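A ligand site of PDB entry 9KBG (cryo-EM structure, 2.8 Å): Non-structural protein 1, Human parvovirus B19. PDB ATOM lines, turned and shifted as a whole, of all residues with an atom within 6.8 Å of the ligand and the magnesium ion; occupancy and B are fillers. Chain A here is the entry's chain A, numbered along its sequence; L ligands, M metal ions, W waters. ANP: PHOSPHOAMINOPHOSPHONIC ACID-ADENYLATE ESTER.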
ATOM      1  N   GLY A 327     -25.254 -33.229 -28.507  1.00  0.00           N
ATOM      2  CA  GLY A 327     -24.150 -33.734 -27.719  1.00  0.00           C
ATOM      3  C   GLY A 327     -24.496 -33.936 -26.252  1.00  0.00           C
ATOM      4  O   GLY A 327     -25.622 -33.680 -25.808  1.00  0.00           O
ATOM      5  N   PRO A 328     -23.518 -34.403 -25.477  1.00  0.00           N
ATOM      6  CA  PRO A 328     -23.721 -34.582 -24.044  1.00  0.00           C
ATOM      7  C   PRO A 328     -23.894 -33.237 -23.348  1.00  0.00           C
ATOM      8  O   PRO A 328     -23.587 -32.190 -23.927  1.00  0.00           O
ATOM      9  CB  PRO A 328     -22.422 -35.271 -23.591  1.00  0.00           C
ATOM     10  CG  PRO A 328     -21.878 -35.909 -24.821  1.00  0.00           C
ATOM     11  CD  PRO A 328     -22.242 -34.977 -25.939  1.00  0.00           C
ATOM     12  N   PRO A 329     -24.400 -33.231 -22.107  1.00  0.00           N
ATOM     13  CA  PRO A 329     -24.645 -31.958 -21.424  1.00  0.00           C
ATOM     14  C   PRO A 329     -23.365 -31.195 -21.124  1.00  0.00           C
ATOM     15  O   PRO A 329     -22.287 -31.765 -21.014  1.00  0.00           O
ATOM     16  CB  PRO A 329     -25.355 -32.381 -20.128  1.00  0.00           C
ATOM     17  CG  PRO A 329     -24.994 -33.814 -19.948  1.00  0.00           C
ATOM     18  CD  PRO A 329     -24.873 -34.379 -21.321  1.00  0.00           C
ATOM     19  N   SER A 330     -23.518 -29.868 -21.005  1.00  0.00           N
ATOM     20  CA  SER A 330     -22.427 -28.954 -20.678  1.00  0.00           C
ATOM     21  C   SER A 330     -21.303 -29.021 -21.718  1.00  0.00           C
ATOM     22  O   SER A 330     -20.144 -29.310 -21.404  1.00  0.00           O
ATOM     23  CB  SER A 330     -21.891 -29.218 -19.272  1.00  0.00           C
ATOM     24  OG  SER A 330     -22.860 -28.920 -18.296  1.00  0.00           O
ATOM     25  N   THR A 331     -21.537 -28.692 -22.958  1.00  0.00           N
ATOM     26  CA  THR A 331     -20.546 -28.805 -24.054  1.00  0.00           C
ATOM     27  C   THR A 331     -20.605 -27.500 -24.863  1.00  0.00           C
ATOM     28  O   THR A 331     -19.935 -27.449 -25.895  1.00  0.00           O
ATOM     29  CB  THR A 331     -20.744 -30.105 -24.855  1.00  0.00           C
ATOM     30  OG1 THR A 331     -22.104 -30.242 -25.246  1.00  0.00           O
ATOM     31  CG2 THR A 331     -20.338 -31.343 -24.089  1.00  0.00           C
ATOM     32  N   GLY A 332     -21.410 -26.500 -24.448  1.00  0.00           N
ATOM     33  CA  GLY A 332     -21.482 -25.176 -25.067  1.00  0.00           C
ATOM     34  C   GLY A 332     -22.651 -24.921 -25.986  1.00  0.00           C
ATOM     35  O   GLY A 332     -22.675 -23.830 -26.499  1.00  0.00           O
ATOM     36  N   LYS A 333     -23.603 -25.818 -26.168  1.00  0.00           N
ATOM     37  CA  LYS A 333     -24.686 -25.702 -27.177  1.00  0.00           C
ATOM     38  C   LYS A 333     -25.573 -24.494 -26.917  1.00  0.00           C
ATOM     39  O   LYS A 333     -25.540 -23.645 -27.708  1.00  0.00           O
ATOM     40  CB  LYS A 333     -25.422 -27.045 -27.290  1.00  0.00           C
ATOM     41  CG  LYS A 333     -24.573 -28.228 -27.717  1.00  0.00           C
ATOM     42  CD  LYS A 333     -25.244 -29.573 -27.505  1.00  0.00           C
ATOM     43  CE  LYS A 333     -26.225 -29.615 -26.365  1.00  0.00           C
ATOM     44  NZ  LYS A 333     -25.611 -30.087 -25.108  1.00  0.00           N
ATOM     45  N   THR A 334     -26.314 -24.411 -25.843  1.00  0.00           N
ATOM     46  CA  THR A 334     -27.108 -23.188 -25.587  1.00  0.00           C
ATOM     47  C   THR A 334     -26.264 -21.925 -25.754  1.00  0.00           C
ATOM     48  O   THR A 334     -26.741 -21.028 -26.412  1.00  0.00           O
ATOM     49  CB  THR A 334     -27.744 -23.110 -24.217  1.00  0.00           C
ATOM     50  OG1 THR A 334     -28.230 -24.423 -23.927  1.00  0.00           O
ATOM     51  CG2 THR A 334     -28.883 -22.135 -24.127  1.00  0.00           C
ATOM     52  N   ASN A 335     -25.082 -21.813 -25.152  1.00  0.00           N
ATOM     53  CA  ASN A 335     -24.167 -20.655 -25.314  1.00  0.00           C
ATOM     54  C   ASN A 335     -23.923 -20.277 -26.787  1.00  0.00           C
ATOM     55  O   ASN A 335     -24.192 -19.149 -27.067  1.00  0.00           O
ATOM     56  CB  ASN A 335     -22.895 -20.945 -24.502  1.00  0.00           C
ATOM     57  CG  ASN A 335     -22.768 -20.137 -23.231  1.00  0.00           C
ATOM     58  OD1 ASN A 335     -23.753 -19.572 -22.760  1.00  0.00           O
ATOM     59  ND2 ASN A 335     -21.576 -20.087 -22.682  1.00  0.00           N
ATOM     60  N   LEU A 336     -23.395 -21.102 -27.682  1.00  0.00           N
ATOM     61  CA  LEU A 336     -23.145 -20.662 -29.084  1.00  0.00           C
ATOM     62  C   LEU A 336     -24.442 -20.316 -29.823  1.00  0.00           C
ATOM     63  O   LEU A 336     -24.373 -19.528 -30.759  1.00  0.00           O
ATOM     64  CB  LEU A 336     -22.362 -21.718 -29.877  1.00  0.00           C
ATOM     65  CG  LEU A 336     -22.101 -21.411 -31.343  1.00  0.00           C
ATOM     66  CD1 LEU A 336     -21.244 -20.179 -31.484  1.00  0.00           C
ATOM     67  CD2 LEU A 336     -21.468 -22.590 -32.050  1.00  0.00           C
ATOM     68  N   ASP A 371     -34.890 -25.019 -27.899  1.00  0.00           N
ATOM     69  CA  ASP A 371     -33.917 -25.444 -26.906  1.00  0.00           C
ATOM     70  C   ASP A 371     -34.386 -26.732 -26.227  1.00  0.00           C
ATOM     71  O   ASP A 371     -35.489 -26.769 -25.679  1.00  0.00           O
ATOM     72  CB  ASP A 371     -33.690 -24.352 -25.870  1.00  0.00           C
ATOM     73  CG  ASP A 371     -32.532 -24.658 -24.938  1.00  0.00           C
ATOM     74  OD1 ASP A 371     -31.371 -24.547 -25.379  1.00  0.00           O
ATOM     75  OD2 ASP A 371     -32.788 -25.006 -23.769  1.00  0.00           O
ATOM     76  N   GLU A 372     -33.543 -27.765 -26.272  1.00  0.00           N
ATOM     77  CA  GLU A 372     -33.834 -29.066 -25.681  1.00  0.00           C
ATOM     78  C   GLU A 372     -35.169 -29.610 -26.174  1.00  0.00           C
ATOM     79  O   GLU A 372     -36.060 -29.956 -25.403  1.00  0.00           O
ATOM     80  CB  GLU A 372     -33.800 -29.002 -24.153  1.00  0.00           C
ATOM     81  CG  GLU A 372     -32.403 -28.803 -23.568  1.00  0.00           C
ATOM     82  CD  GLU A 372     -31.463 -29.942 -23.899  1.00  0.00           C
ATOM     83  OE1 GLU A 372     -30.252 -29.687 -24.080  1.00  0.00           O
ATOM     84  OE2 GLU A 372     -31.924 -31.105 -23.983  1.00  0.00           O
ATOM     85  N   THR A 412     -31.166 -27.276 -30.339  1.00  0.00           N
ATOM     86  CA  THR A 412     -30.220 -27.975 -29.476  1.00  0.00           C
ATOM     87  C   THR A 412     -30.967 -29.068 -28.729  1.00  0.00           C
ATOM     88  O   THR A 412     -32.100 -28.866 -28.282  1.00  0.00           O
ATOM     89  CB  THR A 412     -29.560 -27.014 -28.474  1.00  0.00           C
ATOM     90  OG1 THR A 412     -30.477 -26.716 -27.413  1.00  0.00           O
ATOM     91  CG2 THR A 412     -29.142 -25.727 -29.160  1.00  0.00           C
ATOM     92  N   SER A 413     -30.334 -30.235 -28.605  1.00  0.00           N
ATOM     93  CA  SER A 413     -30.980 -31.369 -27.953  1.00  0.00           C
ATOM     94  C   SER A 413     -29.930 -32.296 -27.356  1.00  0.00           C
ATOM     95  O   SER A 413     -28.748 -32.233 -27.706  1.00  0.00           O
ATOM     96  CB  SER A 413     -31.858 -32.145 -28.939  1.00  0.00           C
ATOM     97  OG  SER A 413     -31.094 -33.044 -29.713  1.00  0.00           O
ATOM     98  N   ASN A 414     -30.378 -33.143 -26.426  1.00  0.00           N
ATOM     99  CA  ASN A 414     -29.538 -34.151 -25.800  1.00  0.00           C
ATOM    100  C   ASN A 414     -29.712 -35.541 -26.396  1.00  0.00           C
ATOM    101  O   ASN A 414     -28.911 -36.430 -26.114  1.00  0.00           O
ATOM    102  CB  ASN A 414     -29.805 -34.215 -24.295  1.00  0.00           C
ATOM    103  CG  ASN A 414     -28.860 -33.347 -23.493  1.00  0.00           C
ATOM    104  OD1 ASN A 414     -27.678 -33.224 -23.830  1.00  0.00           O
ATOM    105  ND2 ASN A 414     -29.359 -32.753 -22.423  1.00  0.00           N
ATOM    106  N   PHE A 443     -21.243 -31.949 -30.373  1.00  0.00           N
ATOM    107  CA  PHE A 443     -20.511 -31.241 -29.329  1.00  0.00           C
ATOM    108  C   PHE A 443     -20.183 -32.253 -28.231  1.00  0.00           C
ATOM    109  O   PHE A 443     -20.951 -32.443 -27.287  1.00  0.00           O
ATOM    110  CB  PHE A 443     -21.327 -30.068 -28.775  1.00  0.00           C
ATOM    111  CG  PHE A 443     -21.228 -28.816 -29.597  1.00  0.00           C
ATOM    112  CD1 PHE A 443     -21.375 -28.852 -30.975  1.00  0.00           C
ATOM    113  CD2 PHE A 443     -21.011 -27.589 -28.989  1.00  0.00           C
ATOM    114  CE1 PHE A 443     -21.294 -27.710 -31.734  1.00  0.00           C
ATOM    115  CE2 PHE A 443     -20.925 -26.431 -29.740  1.00  0.00           C
ATOM    116  CZ  PHE A 443     -21.068 -26.495 -31.107  1.00  0.00           C
ATOM    117  N   ARG A 446     -16.411 -31.923 -23.178  1.00  0.00           N
ATOM    118  CA  ARG A 446     -16.962 -31.125 -22.093  1.00  0.00           C
ATOM    119  C   ARG A 446     -16.162 -29.843 -21.914  1.00  0.00           C
ATOM    120  O   ARG A 446     -14.941 -29.814 -22.094  1.00  0.00           O
ATOM    121  CB  ARG A 446     -16.987 -31.941 -20.808  1.00  0.00           C
ATOM    122  CG  ARG A 446     -17.399 -31.175 -19.562  1.00  0.00           C
ATOM    123  CD  ARG A 446     -18.202 -32.043 -18.608  1.00  0.00           C
ATOM    124  NE  ARG A 446     -18.769 -31.275 -17.508  1.00  0.00           N
ATOM    125  CZ  ARG A 446     -19.910 -31.576 -16.897  1.00  0.00           C
ATOM    126  NH1 ARG A 446     -20.618 -32.638 -17.249  1.00  0.00           N
ATOM    127  NH2 ARG A 446     -20.332 -30.802 -15.903  1.00  0.00           N
ATOM    128  N   CYS A 447     -16.865 -28.770 -21.554  1.00  0.00           N
ATOM    129  CA  CYS A 447     -16.268 -27.450 -21.383  1.00  0.00           C
ATOM    130  C   CYS A 447     -15.899 -27.212 -19.926  1.00  0.00           C
ATOM    131  O   CYS A 447     -16.423 -27.850 -19.014  1.00  0.00           O
ATOM    132  CB  CYS A 447     -17.222 -26.362 -21.865  1.00  0.00           C
ATOM    133  SG  CYS A 447     -17.521 -26.356 -23.645  1.00  0.00           S
ATOM    134  N   SER A 448     -14.973 -26.272 -19.734  1.00  0.00           N
ATOM    135  CA  SER A 448     -14.503 -25.883 -18.412  1.00  0.00           C
ATOM    136  C   SER A 448     -15.616 -25.221 -17.608  1.00  0.00           C
ATOM    137  O   SER A 448     -16.473 -24.536 -18.188  1.00  0.00           O
ATOM    138  CB  SER A 448     -13.301 -24.941 -18.532  1.00  0.00           C
ATOM    139  OG  SER A 448     -12.882 -24.475 -17.265  1.00  0.00           O
ATOM    140  N   PRO A 449     -15.658 -25.407 -16.292  1.00  0.00           N
ATOM    141  CA  PRO A 449     -16.702 -24.771 -15.477  1.00  0.00           C
ATOM    142  C   PRO A 449     -16.576 -23.260 -15.351  1.00  0.00           C
ATOM    143  O   PRO A 449     -17.437 -22.642 -14.719  1.00  0.00           O
ATOM    144  CB  PRO A 449     -16.511 -25.448 -14.104  1.00  0.00           C
ATOM    145  CG  PRO A 449     -15.696 -26.669 -14.364  1.00  0.00           C
ATOM    146  CD  PRO A 449     -14.799 -26.301 -15.497  1.00  0.00           C
ATOM    147  N   ASP A 450     -15.536 -22.645 -15.923  1.00  0.00           N
ATOM    148  CA  ASP A 450     -15.329 -21.201 -15.868  1.00  0.00           C
ATOM    149  C   ASP A 450     -15.136 -20.693 -17.291  1.00  0.00           C
ATOM    150  O   ASP A 450     -14.277 -19.857 -17.579  1.00  0.00           O
ATOM    151  CB  ASP A 450     -14.138 -20.838 -14.966  1.00  0.00           C
ATOM    152  CG  ASP A 450     -14.444 -20.991 -13.501  1.00  0.00           C
ATOM    153  OD1 ASP A 450     -15.619 -20.783 -13.104  1.00  0.00           O
ATOM    154  OD2 ASP A 450     -13.525 -21.326 -12.725  1.00  0.00           O
ATOM    155  N   MET A 451     -15.957 -21.203 -18.210  1.00  0.00           N
ATOM    156  CA  MET A 451     -15.937 -20.792 -19.607  1.00  0.00           C
ATOM    157  C   MET A 451     -16.418 -19.360 -19.820  1.00  0.00           C
ATOM    158  O   MET A 451     -15.829 -18.635 -20.625  1.00  0.00           O
ATOM    159  CB  MET A 451     -16.807 -21.737 -20.445  1.00  0.00           C
ATOM    160  CG  MET A 451     -16.782 -21.439 -21.938  1.00  0.00           C
ATOM    161  SD  MET A 451     -17.743 -22.633 -22.894  1.00  0.00           S
ATOM    162  CE  MET A 451     -17.589 -21.926 -24.541  1.00  0.00           C
ATOM    163  N   GLY A 452     -17.455 -18.943 -19.119  1.00  0.00           N
ATOM    164  CA  GLY A 452     -17.976 -17.595 -19.251  1.00  0.00           C
ATOM    165  C   GLY A 452     -19.077 -17.512 -20.278  1.00  0.00           C
ATOM    166  O   GLY A 452     -19.117 -18.256 -21.261  1.00  0.00           O
ATOM    167  N   LEU A 453     -20.004 -16.586 -20.050  1.00  0.00           N
ATOM    168  CA  LEU A 453     -21.121 -16.398 -20.973  1.00  0.00           C
ATOM    169  C   LEU A 453     -20.635 -15.683 -22.225  1.00  0.00           C
ATOM    170  O   LEU A 453     -19.939 -14.664 -22.142  1.00  0.00           O
ATOM    171  CB  LEU A 453     -22.230 -15.598 -20.291  1.00  0.00           C
ATOM    172  CG  LEU A 453     -23.500 -15.359 -21.096  1.00  0.00           C
ATOM    173  CD1 LEU A 453     -24.172 -16.679 -21.428  1.00  0.00           C
ATOM    174  CD2 LEU A 453     -24.447 -14.445 -20.338  1.00  0.00           C
ATOM    175  N   LEU A 454     -21.009 -16.219 -23.385  1.00  0.00           N
ATOM    176  CA  LEU A 454     -20.572 -15.626 -24.648  1.00  0.00           C
ATOM    177  C   LEU A 454     -21.262 -14.297 -24.890  1.00  0.00           C
ATOM    178  O   LEU A 454     -22.340 -14.012 -24.339  1.00  0.00           O
ATOM    179  CB  LEU A 454     -20.848 -16.588 -25.800  1.00  0.00           C
ATOM    180  CG  LEU A 454     -20.099 -17.921 -25.735  1.00  0.00           C
ATOM    181  CD1 LEU A 454     -20.602 -18.880 -26.803  1.00  0.00           C
ATOM    182  CD2 LEU A 454     -18.601 -17.703 -25.866  1.00  0.00           C
HETATM  183  PG  ANP L   1     -26.951 -29.028 -21.511  1.00  0.00           P
HETATM  184  O1G ANP L   1     -26.850 -29.518 -20.121  1.00  0.00           O
HETATM  185  O2G ANP L   1     -26.928 -30.111 -22.526  1.00  0.00           O
HETATM  186  O3G ANP L   1     -28.100 -28.114 -21.682  1.00  0.00           O
HETATM  187  PB  ANP L   1     -25.206 -27.029 -22.819  1.00  0.00           P
HETATM  188  O1B ANP L   1     -24.303 -27.569 -23.851  1.00  0.00           O
HETATM  189  O2B ANP L   1     -26.464 -26.361 -23.205  1.00  0.00           O
HETATM  190  N3B ANP L   1     -25.619 -28.186 -21.807  1.00  0.00           N
HETATM  191  PA  ANP L   1     -24.164 -24.470 -21.616  1.00  0.00           P
HETATM  192  O1A ANP L   1     -25.231 -23.974 -20.729  1.00  0.00           O
HETATM  193  O2A ANP L   1     -23.920 -23.806 -22.916  1.00  0.00           O
HETATM  194  O3A ANP L   1     -24.368 -26.037 -21.874  1.00  0.00           O
HETATM  195  O5' ANP L   1     -22.777 -24.465 -20.826  1.00  0.00           O
HETATM  196  C5' ANP L   1     -21.617 -24.404 -21.696  1.00  0.00           C
HETATM  197  C4' ANP L   1     -20.414 -23.933 -20.915  1.00  0.00           C
HETATM  198  O4' ANP L   1     -20.486 -22.492 -20.737  1.00  0.00           O
HETATM  199  C3' ANP L   1     -20.237 -24.541 -19.526  1.00  0.00           C
HETATM  200  O3' ANP L   1     -18.895 -24.997 -19.358  1.00  0.00           O
HETATM  201  C2' ANP L   1     -20.621 -23.430 -18.551  1.00  0.00           C
HETATM  202  O2' ANP L   1     -19.787 -23.339 -17.432  1.00  0.00           O
HETATM  203  C1' ANP L   1     -20.531 -22.147 -19.375  1.00  0.00           C
HETATM  204  N9  ANP L   1     -21.721 -21.369 -19.127  1.00  0.00           N
HETATM  205  C8  ANP L   1     -22.999 -21.713 -19.443  1.00  0.00           C
HETATM  206  N7  ANP L   1     -23.877 -20.819 -19.042  1.00  0.00           N
HETATM  207  C5  ANP L   1     -23.119 -19.854 -18.407  1.00  0.00           C
HETATM  208  C6  ANP L   1     -23.463 -18.656 -17.758  1.00  0.00           C
HETATM  209  N6  ANP L   1     -24.702 -18.215 -17.650  1.00  0.00           N
HETATM  210  N1  ANP L   1     -22.458 -17.930 -17.232  1.00  0.00           N
HETATM  211  C2  ANP L   1     -21.201 -18.384 -17.352  1.00  0.00           C
HETATM  212  N3  ANP L   1     -20.768 -19.498 -17.941  1.00  0.00           N
HETATM  213  C4  ANP L   1     -21.787 -20.197 -18.447  1.00  0.00           C
HETATM  214 MG    MG M   1     -28.453 -26.235 -22.808  1.00  0.00          MG
HETATM  215  O   HOH W   1     -28.298 -25.081 -21.006  1.00  0.00           O
HETATM  216  O   HOH W   2     -28.820 -27.486 -24.678  1.00  0.00           O
HETATM  217  O   HOH W   3     -30.600 -26.034 -22.705  1.00  0.00           O
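OD1 of Asp 371 sits close to OG1 of Thr 334, at 3.5 Å.
The backbone NH of Cys 447 sits at hydrogen-bond distance from the backbone carbonyl oxygen of Ser 330.
O of Thr 331 lies within hydrogen-bond range of SG of Cys 447, 3.5 Å away.
The side-chain hydroxyl (OG1) of Thr 331 sits at hydrogen-bond distance from the backbone carbonyl oxygen (O) of Phe 443 (3.2 Å).
The side-chain amide nitrogen (ND2) of Asn 335 lies within hydrogen-bond range of the backbone carbonyl oxygen (O) of Gly 452.
The side-chain amide nitrogen of Asn 414 is in hydrogen-bond range of the side-chain carboxylate of Glu 372 (3.4 Å).
O of Gly 327 lies close to OD1 of Asn 414 (2.9 Å).
The backbone NH (N) of Glu 372 is in hydrogen-bond range of the backbone carbonyl oxygen (O) of Thr 412, at 2.7 Å.
An oxygen (O2B) of the ligand sits close to the backbone NH of Thr 334 (3.3 Å).
An oxygen (O3') of the ligand lies within hydrogen-bond range of the backbone carbonyl oxygen (O) of Ser 448 (2.7 Å).
N of Ser 330 sits at hydrogen-bond distance from O1G of the ligand, 3.5 Å away.
The backbone NH of Lys 333 lies within hydrogen-bond range of an oxygen (O1B) of the ligand (3.0 Å).
NZ of Lys 333 lies within salt-bridge range of O2G of the ligand, 2.9 Å away.
The backbone NH (N) of Thr 331 sits at hydrogen-bond distance from an oxygen (O1B) of the ligand.
The backbone NH (N) of Gly 332 is in hydrogen-bond range of an oxygen (O1B) of the ligand, 3.1 Å away.
N of Asn 335 is in hydrogen-bond range of O2A of the ligand, 3.2 Å away.
ND2 of Asn 335 sits at hydrogen-bond distance from O4' of the ligand (3.3 Å).
The side-chain amide oxygen of Asn 414 lies close to an oxygen (O2G) of the ligand (3.5 Å).
One residue has an atom within 4 Å of the magnesium ion: Thr 334.
Water W2 lies within hydrogen-bond range of OE1 of Glu 372 and OG1 of Thr 412.
The side-chain sulfur of Met 451 lies close to an oxygen (O4') of the ligand (3.5 Å).
CA of Pro 329 touches O2G of the ligand, 3.1 Å away.
Glu 372 touches the ligand (OE1 to O3G, 3.6 Å).
Cys 447 touches the ligand (CB to O3', 3.3 Å).
Pro 449 touches the ligand (O to O2', 3.7 Å).
Gly 452 touches the ligand.
N of Leu 453 touches C2 of the ligand (3.5 Å).
Hydrophobic or aromatic side chains within 4 Å of the ligand: Pro 329, Met 451 and Leu 453.
Within 4 Å of the ligand: Pro 329, Ser 330, Thr 331, Gly 332, Lys 333, Thr 334, Asn 335, Glu 372, Asn 414, Cys 447, Ser 448, Pro 449, Met 451, Gly 452 and Leu 453.
The magnesium ion is bound by O2B of the ligand (2.0 Å), OG1 of Thr 334 (2.1 Å), water W1 (2.1 Å), water W3 (2.2 Å), O3G of the ligand (2.2 Å) and water W2 (2.3 Å).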
